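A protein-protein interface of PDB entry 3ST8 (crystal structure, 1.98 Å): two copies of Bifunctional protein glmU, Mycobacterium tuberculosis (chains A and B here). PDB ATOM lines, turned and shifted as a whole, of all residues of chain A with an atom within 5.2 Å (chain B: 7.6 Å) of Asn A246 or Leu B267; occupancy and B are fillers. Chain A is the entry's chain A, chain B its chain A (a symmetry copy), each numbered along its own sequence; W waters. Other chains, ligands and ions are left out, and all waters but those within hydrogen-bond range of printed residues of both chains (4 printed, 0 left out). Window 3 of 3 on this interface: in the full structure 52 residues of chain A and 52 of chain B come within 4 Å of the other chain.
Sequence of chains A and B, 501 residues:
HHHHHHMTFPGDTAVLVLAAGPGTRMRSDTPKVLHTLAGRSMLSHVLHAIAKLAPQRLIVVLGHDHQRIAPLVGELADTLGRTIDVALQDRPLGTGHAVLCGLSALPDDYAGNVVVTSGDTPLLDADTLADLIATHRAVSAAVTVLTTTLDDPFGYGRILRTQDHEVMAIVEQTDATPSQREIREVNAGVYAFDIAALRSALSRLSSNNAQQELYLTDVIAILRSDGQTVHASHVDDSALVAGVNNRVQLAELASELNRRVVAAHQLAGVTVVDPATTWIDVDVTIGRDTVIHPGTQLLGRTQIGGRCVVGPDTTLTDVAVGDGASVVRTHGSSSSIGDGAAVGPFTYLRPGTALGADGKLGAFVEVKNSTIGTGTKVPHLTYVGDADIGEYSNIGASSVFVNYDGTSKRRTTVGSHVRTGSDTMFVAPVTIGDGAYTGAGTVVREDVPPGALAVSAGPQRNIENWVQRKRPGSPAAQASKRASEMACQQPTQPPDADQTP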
ATOM      1  N   ARG A  25      -5.914  21.013 -15.787  1.00  0.00           N
ATOM      2  CA  ARG A  25      -4.700  21.501 -16.482  1.00  0.00           C
ATOM      3  C   ARG A  25      -3.548  20.405 -16.527  1.00  0.00           C
ATOM      4  O   ARG A  25      -2.561  20.506 -17.323  1.00  0.00           O
ATOM      5  CB  ARG A  25      -4.248  22.796 -15.814  1.00  0.00           C
ATOM      6  CG  ARG A  25      -5.085  23.969 -16.323  1.00  0.00           C
ATOM      7  CD  ARG A  25      -4.794  25.158 -15.486  1.00  0.00           C
ATOM      8  NE  ARG A  25      -4.683  24.941 -14.011  1.00  0.00           N
ATOM      9  CZ  ARG A  25      -5.499  25.425 -13.072  1.00  0.00           C
ATOM     10  NH1 ARG A  25      -6.580  26.148 -13.410  1.00  0.00           N
ATOM     11  NH2 ARG A  25      -5.261  25.214 -11.787  1.00  0.00           N
ATOM     12  N   MET A  26      -3.747  19.331 -15.784  1.00  0.00           N
ATOM     13  CA  MET A  26      -2.852  18.148 -15.931  1.00  0.00           C
ATOM     14  C   MET A  26      -3.095  17.429 -17.218  1.00  0.00           C
ATOM     15  O   MET A  26      -2.227  16.704 -17.712  1.00  0.00           O
ATOM     16  CB  MET A  26      -3.016  17.152 -14.780  1.00  0.00           C
ATOM     17  CG  MET A  26      -2.673  17.791 -13.420  1.00  0.00           C
ATOM     18  SD  MET A  26      -0.896  18.239 -13.253  1.00  0.00           S
ATOM     19  CE  MET A  26      -0.205  16.617 -13.246  1.00  0.00           C
ATOM     20  N   ARG A  27      -4.323  17.553 -17.747  1.00  0.00           N
ATOM     21  CA  ARG A  27      -4.725  16.776 -18.879  1.00  0.00           C
ATOM     22  C   ARG A  27      -4.424  15.292 -18.728  1.00  0.00           C
ATOM     23  O   ARG A  27      -3.778  14.654 -19.637  1.00  0.00           O
ATOM     24  CB  ARG A  27      -4.059  17.279 -20.182  1.00  0.00           C
ATOM     25  CG  ARG A  27      -4.260  18.695 -20.538  1.00  0.00           C
ATOM     26  CD  ARG A  27      -5.591  19.006 -21.076  1.00  0.00           C
ATOM     27  NE  ARG A  27      -5.593  20.468 -20.945  1.00  0.00           N
ATOM     28  CZ  ARG A  27      -6.645  21.265 -20.740  1.00  0.00           C
ATOM     29  NH1 ARG A  27      -7.913  20.797 -20.723  1.00  0.00           N
ATOM     30  NH2 ARG A  27      -6.396  22.559 -20.552  1.00  0.00           N
ATOM     31  N   VAL A 244       1.756  22.802  -7.962  1.00  0.00           N
ATOM     32  CA  VAL A 244       1.745  22.053  -9.179  1.00  0.00           C
ATOM     33  C   VAL A 244       0.297  21.981  -9.799  1.00  0.00           C
ATOM     34  O   VAL A 244      -0.587  21.178  -9.333  1.00  0.00           O
ATOM     35  CB  VAL A 244       2.202  20.703  -8.912  1.00  0.00           C
ATOM     36  CG1 VAL A 244       2.077  19.856 -10.155  1.00  0.00           C
ATOM     37  CG2 VAL A 244       3.713  20.782  -8.323  1.00  0.00           C
ATOM     38  N   ASN A 245       0.070  22.806 -10.836  1.00  0.00           N
ATOM     39  CA  ASN A 245      -1.234  22.699 -11.593  1.00  0.00           C
ATOM     40  C   ASN A 245      -1.103  22.023 -12.980  1.00  0.00           C
ATOM     41  O   ASN A 245      -2.127  21.671 -13.591  1.00  0.00           O
ATOM     42  CB  ASN A 245      -1.808  24.144 -11.743  1.00  0.00           C
ATOM     43  CG  ASN A 245      -2.276  24.735 -10.431  1.00  0.00           C
ATOM     44  OD1 ASN A 245      -2.557  23.957  -9.491  1.00  0.00           O
ATOM     45  ND2 ASN A 245      -2.397  26.155 -10.329  1.00  0.00           N
ATOM     46  N   ASN A 246       0.121  21.823 -13.538  1.00  0.00           N
ATOM     47  CA  ASN A 246       0.218  21.190 -14.816  1.00  0.00           C
ATOM     48  C   ASN A 246       1.578  20.389 -14.837  1.00  0.00           C
ATOM     49  O   ASN A 246       2.333  20.455 -13.844  1.00  0.00           O
ATOM     50  CB  ASN A 246       0.175  22.305 -15.952  1.00  0.00           C
ATOM     51  CG  ASN A 246       1.310  23.328 -15.791  1.00  0.00           C
ATOM     52  OD1 ASN A 246       2.452  22.971 -15.544  1.00  0.00           O
ATOM     53  ND2 ASN A 246       1.003  24.588 -15.907  1.00  0.00           N
ATOM     54  N   ARG A 247       1.822  19.694 -15.946  1.00  0.00           N
ATOM     55  CA  ARG A 247       3.012  18.827 -16.034  1.00  0.00           C
ATOM     56  C   ARG A 247       4.332  19.611 -16.157  1.00  0.00           C
ATOM     57  O   ARG A 247       5.393  19.054 -15.855  1.00  0.00           O
ATOM     58  CB  ARG A 247       2.796  17.923 -17.181  1.00  0.00           C
ATOM     59  CG  ARG A 247       1.720  16.872 -16.798  1.00  0.00           C
ATOM     60  CD  ARG A 247       1.688  15.636 -17.664  1.00  0.00           C
ATOM     61  NE  ARG A 247       0.342  15.151 -17.921  1.00  0.00           N
ATOM     62  CZ  ARG A 247      -0.084  13.927 -18.035  1.00  0.00           C
ATOM     63  NH1 ARG A 247       0.646  12.831 -17.896  1.00  0.00           N
ATOM     64  NH2 ARG A 247      -1.321  13.798 -18.344  1.00  0.00           N
ATOM     65  N   VAL A 248       4.300  20.889 -16.601  1.00  0.00           N
ATOM     66  CA  VAL A 248       5.516  21.683 -16.635  1.00  0.00           C
ATOM     67  C   VAL A 248       5.963  21.990 -15.205  1.00  0.00           C
ATOM     68  O   VAL A 248       7.141  21.792 -14.831  1.00  0.00           O
ATOM     69  CB  VAL A 248       5.285  23.041 -17.377  1.00  0.00           C
ATOM     70  CG1 VAL A 248       6.536  24.000 -17.194  1.00  0.00           C
ATOM     71  CG2 VAL A 248       4.944  22.752 -18.837  1.00  0.00           C
ATOM     72  N   GLN A 249       5.008  22.384 -14.363  1.00  0.00           N
ATOM     73  CA  GLN A 249       5.342  22.703 -12.945  1.00  0.00           C
ATOM     74  C   GLN A 249       5.751  21.421 -12.237  1.00  0.00           C
ATOM     75  O   GLN A 249       6.602  21.449 -11.317  1.00  0.00           O
ATOM     76  CB  GLN A 249       4.082  23.335 -12.257  1.00  0.00           C
ATOM     77  CG  GLN A 249       3.867  24.805 -12.850  1.00  0.00           C
ATOM     78  CD  GLN A 249       2.645  25.515 -12.151  1.00  0.00           C
ATOM     79  OE1 GLN A 249       1.740  24.856 -11.777  1.00  0.00           O
ATOM     80  NE2 GLN A 249       2.712  26.796 -11.955  1.00  0.00           N
ATOM     81  N   LEU A 250       5.097  20.341 -12.605  1.00  0.00           N
ATOM     82  CA  LEU A 250       5.403  19.121 -11.894  1.00  0.00           C
ATOM     83  C   LEU A 250       6.901  18.750 -12.213  1.00  0.00           C
ATOM     84  O   LEU A 250       7.613  18.363 -11.302  1.00  0.00           O
ATOM     85  CB  LEU A 250       4.645  17.929 -12.454  1.00  0.00           C
ATOM     86  CG  LEU A 250       4.941  16.551 -11.816  1.00  0.00           C
ATOM     87  CD1 LEU A 250       4.871  16.649 -10.225  1.00  0.00           C
ATOM     88  CD2 LEU A 250       4.109  15.464 -12.427  1.00  0.00           C
ATOM     89  N   ARG B 260      10.872  24.502 -25.454  1.00  0.00           N
ATOM     90  CA  ARG B 260       9.514  24.951 -25.803  1.00  0.00           C
ATOM     91  C   ARG B 260       8.702  23.812 -26.394  1.00  0.00           C
ATOM     92  O   ARG B 260       7.473  23.728 -26.203  1.00  0.00           O
ATOM     93  CB  ARG B 260       9.656  26.095 -26.859  1.00  0.00           C
ATOM     94  CG  ARG B 260      10.189  27.376 -26.125  1.00  0.00           C
ATOM     95  CD  ARG B 260      10.566  28.523 -27.201  1.00  0.00           C
ATOM     96  NE  ARG B 260      11.206  29.606 -26.486  1.00  0.00           N
ATOM     97  CZ  ARG B 260      10.910  30.925 -26.541  1.00  0.00           C
ATOM     98  NH1 ARG B 260      10.084  31.403 -27.449  1.00  0.00           N
ATOM     99  NH2 ARG B 260      11.547  31.782 -25.681  1.00  0.00           N
ATOM    100  N   VAL B 261       9.350  22.988 -27.227  1.00  0.00           N
ATOM    101  CA  VAL B 261       8.669  21.821 -27.831  1.00  0.00           C
ATOM    102  C   VAL B 261       8.193  20.886 -26.709  1.00  0.00           C
ATOM    103  O   VAL B 261       7.012  20.414 -26.680  1.00  0.00           O
ATOM    104  CB  VAL B 261       9.623  21.066 -28.801  1.00  0.00           C
ATOM    105  CG1 VAL B 261       8.989  19.738 -29.287  1.00  0.00           C
ATOM    106  CG2 VAL B 261       9.796  21.994 -30.097  1.00  0.00           C
ATOM    107  N   VAL B 262       9.124  20.580 -25.798  1.00  0.00           N
ATOM    108  CA  VAL B 262       8.754  19.703 -24.631  1.00  0.00           C
ATOM    109  C   VAL B 262       7.628  20.300 -23.791  1.00  0.00           C
ATOM    110  O   VAL B 262       6.701  19.561 -23.472  1.00  0.00           O
ATOM    111  CB  VAL B 262      10.026  19.482 -23.694  1.00  0.00           C
ATOM    112  CG1 VAL B 262       9.591  18.744 -22.374  1.00  0.00           C
ATOM    113  CG2 VAL B 262      11.029  18.623 -24.525  1.00  0.00           C
ATOM    114  N   ALA B 263       7.713  21.606 -23.481  1.00  0.00           N
ATOM    115  CA  ALA B 263       6.689  22.230 -22.684  1.00  0.00           C
ATOM    116  C   ALA B 263       5.327  22.127 -23.345  1.00  0.00           C
ATOM    117  O   ALA B 263       4.327  21.858 -22.660  1.00  0.00           O
ATOM    118  CB  ALA B 263       7.044  23.778 -22.329  1.00  0.00           C
ATOM    119  N   ALA B 264       5.257  22.330 -24.672  1.00  0.00           N
ATOM    120  CA  ALA B 264       3.979  22.129 -25.342  1.00  0.00           C
ATOM    121  C   ALA B 264       3.397  20.704 -25.163  1.00  0.00           C
ATOM    122  O   ALA B 264       2.177  20.525 -24.949  1.00  0.00           O
ATOM    123  CB  ALA B 264       4.117  22.465 -26.903  1.00  0.00           C
ATOM    124  N   HIS B 265       4.250  19.678 -25.253  1.00  0.00           N
ATOM    125  CA  HIS B 265       3.745  18.340 -25.048  1.00  0.00           C
ATOM    126  C   HIS B 265       3.327  18.165 -23.563  1.00  0.00           C
ATOM    127  O   HIS B 265       2.288  17.520 -23.311  1.00  0.00           O
ATOM    128  CB  HIS B 265       4.837  17.264 -25.389  1.00  0.00           C
ATOM    129  CG  HIS B 265       5.089  17.136 -26.850  1.00  0.00           C
ATOM    130  ND1 HIS B 265       4.149  16.606 -27.698  1.00  0.00           N
ATOM    131  CD2 HIS B 265       6.144  17.497 -27.622  1.00  0.00           C
ATOM    132  CE1 HIS B 265       4.598  16.654 -28.951  1.00  0.00           C
ATOM    133  NE2 HIS B 265       5.814  17.207 -28.932  1.00  0.00           N
ATOM    134  N   GLN B 266       4.099  18.689 -22.602  1.00  0.00           N
ATOM    135  CA  GLN B 266       3.684  18.567 -21.190  1.00  0.00           C
ATOM    136  C   GLN B 266       2.295  19.212 -20.960  1.00  0.00           C
ATOM    137  O   GLN B 266       1.384  18.628 -20.258  1.00  0.00           O
ATOM    138  CB  GLN B 266       4.662  19.300 -20.288  1.00  0.00           C
ATOM    139  CG  GLN B 266       6.053  18.500 -20.254  1.00  0.00           C
ATOM    140  CD  GLN B 266       7.052  19.345 -19.544  1.00  0.00           C
ATOM    141  OE1 GLN B 266       7.431  20.398 -20.050  1.00  0.00           O
ATOM    142  NE2 GLN B 266       7.519  18.866 -18.385  1.00  0.00           N
ATOM    143  N   LEU B 267       2.119  20.423 -21.458  1.00  0.00           N
ATOM    144  CA  LEU B 267       0.793  21.074 -21.297  1.00  0.00           C
ATOM    145  C   LEU B 267      -0.319  20.289 -22.008  1.00  0.00           C
ATOM    146  O   LEU B 267      -1.502  20.368 -21.600  1.00  0.00           O
ATOM    147  CB  LEU B 267       0.885  22.528 -21.827  1.00  0.00           C
ATOM    148  CG  LEU B 267       1.791  23.413 -20.960  1.00  0.00           C
ATOM    149  CD1 LEU B 267       1.912  24.877 -21.546  1.00  0.00           C
ATOM    150  CD2 LEU B 267       1.385  23.499 -19.496  1.00  0.00           C
ATOM    151  N   ALA B 268       0.032  19.548 -23.073  1.00  0.00           N
ATOM    152  CA  ALA B 268      -0.989  18.797 -23.742  1.00  0.00           C
ATOM    153  C   ALA B 268      -1.241  17.481 -23.015  1.00  0.00           C
ATOM    154  O   ALA B 268      -2.070  16.772 -23.455  1.00  0.00           O
ATOM    155  CB  ALA B 268      -0.632  18.494 -25.297  1.00  0.00           C
ATOM    156  N   GLY B 269      -0.475  17.069 -22.000  1.00  0.00           N
ATOM    157  CA  GLY B 269      -0.834  15.813 -21.339  1.00  0.00           C
ATOM    158  C   GLY B 269       0.262  14.727 -21.403  1.00  0.00           C
ATOM    159  O   GLY B 269      -0.036  13.580 -21.124  1.00  0.00           O
ATOM    160  N   VAL B 270       1.519  15.114 -21.671  1.00  0.00           N
ATOM    161  CA  VAL B 270       2.608  14.113 -21.720  1.00  0.00           C
ATOM    162  C   VAL B 270       3.497  14.362 -20.462  1.00  0.00           C
ATOM    163  O   VAL B 270       3.907  15.517 -20.223  1.00  0.00           O
ATOM    164  CB  VAL B 270       3.492  14.277 -23.011  1.00  0.00           C
ATOM    165  CG1 VAL B 270       4.681  13.178 -23.043  1.00  0.00           C
ATOM    166  CG2 VAL B 270       2.563  14.128 -24.265  1.00  0.00           C
ATOM    167  N   THR B 271       3.786  13.322 -19.685  1.00  0.00           N
ATOM    168  CA  THR B 271       4.687  13.521 -18.583  1.00  0.00           C
ATOM    169  C   THR B 271       6.067  13.386 -19.189  1.00  0.00           C
ATOM    170  O   THR B 271       6.416  12.360 -19.788  1.00  0.00           O
ATOM    171  CB  THR B 271       4.481  12.408 -17.510  1.00  0.00           C
ATOM    172  OG1 THR B 271       3.254  12.692 -16.817  1.00  0.00           O
ATOM    173  CG2 THR B 271       5.645  12.298 -16.468  1.00  0.00           C
HETATM  174  O   HOH W   1       6.332  16.430 -17.276  1.00  0.00           O
HETATM  175  O   HOH W   2      -0.057  19.546 -18.134  1.00  0.00           O
HETATM  176  O   HOH W   3      -2.471  22.067 -19.528  1.00  0.00           O
HETATM  177  O   HOH W   4       9.135  21.379 -16.748  1.00  0.00           O
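The backbone carbonyl oxygen of Arg A247 lies within hydrogen-bond range of the side-chain amide nitrogen of Gln B266.
The guanidinium group (NH1) of Arg A247 sits at hydrogen-bond distance from the side-chain hydroxyl (OG1) of Thr B271, 2.8 Å away.
The backbone carbonyl oxygen of Gly B269 lies within hydrogen-bond range of the guanidinium group of Arg A247.
The side-chain sulfur (SD) of Met A26 sits close to the backbone NH (N) of Asn A246 (3.7 Å).
The side-chain amide oxygen (OD1) of Asn A246 is in hydrogen-bond range of the backbone NH (N) of Gln A249, at 2.9 Å.
The backbone carbonyl oxygen (O) of Arg A27 sits at hydrogen-bond distance from the guanidinium group (NH2) of Arg A247 (2.9 Å).
NE of Arg A247 is in hydrogen-bond range of O of Met A26 (3.0 Å).
The backbone NH (N) of Val B270 is in hydrogen-bond range of the backbone carbonyl oxygen (O) of His B265 (3.0 Å).
OD1 of Asn A246 lies within hydrogen-bond range of N of Val A248 (3.0 Å).
Gly B269 touches Met A26.
Leu B267 touches Arg A27.
O of Ala B268 touches CB of Arg A27, 3.9 Å away.
Arg A27 touches Gly B269 (O to CA, 3.6 Å).
Asn A246 touches Leu B267 (CG to CD2, 3.7 Å).
Arg A247 touches Val B270 (CD to O, 3.4 Å).
CG2 of Val A248 touches O of Ala B263, at 3.97 Å.
CG2 of Val A248 touches OE1 of Gln B266 (3.6 Å).
Leu B267 touches Val A248 (CD2 to CG2, 3.7 Å).
Of the printed residues of chain B, Met A26 touches Gly B269.
Val A244 touches none of the printed residues of chain B.
Asn A246 touches one residue of chain B.
Of the printed residues of chain B, Arg A247 touches Gln B266 (3.3 Å), Gly B269 (3.1 Å), Val B270 (3.4 Å) and Thr B271 (2.8 Å).
Gln A249 touches none of the printed residues of chain B.
Of the printed residues of chain A, Gln B266 touches Arg A247 and Val A248.
Leu B267 touches three residues of chain A.
Printed residues of chain A within 4 Å of Thr B271: Arg A247 (2.8 Å).
The nearest residue of chain B that does not touch Asn A246 is Gln B266 (5.7 Å).
The nearest residue of chain A that does not touch Leu B267 is Arg A25 (4.4 Å).
The nearest printed residue of chain B that does not touch Met A26 is Gln B266 (4.8 Å).
Hydrophobic or aromatic side chains of chain B within 4 Å of the printed part of chain A: Leu B267.
Hydrophobic or aromatic side chains of chain A within 4 Å of the printed part of chain B: Val A248.
Among the printed residues, 12 pairs touch across the chains.
No position is printed for both chains.
Of the 12 pairs that touch across the chains among the printed residues, none has its exchanged pair printed and touching as well.
Water W3 bridges O of Arg A25 (2.7 Å) and O of Leu B267 (2.8 Å).
Water W2 lies within hydrogen-bond range of O of Gln B266 (2.7 Å), O of Arg A25 (2.8 Å) and N of Arg A247 (2.9 Å).
Water W4 bridges O of Val A248 (2.8 Å) and NE2 of Gln B266 (3.4 Å).
Water W1 bridges NE2 of Gln B266 and O of Arg A247.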
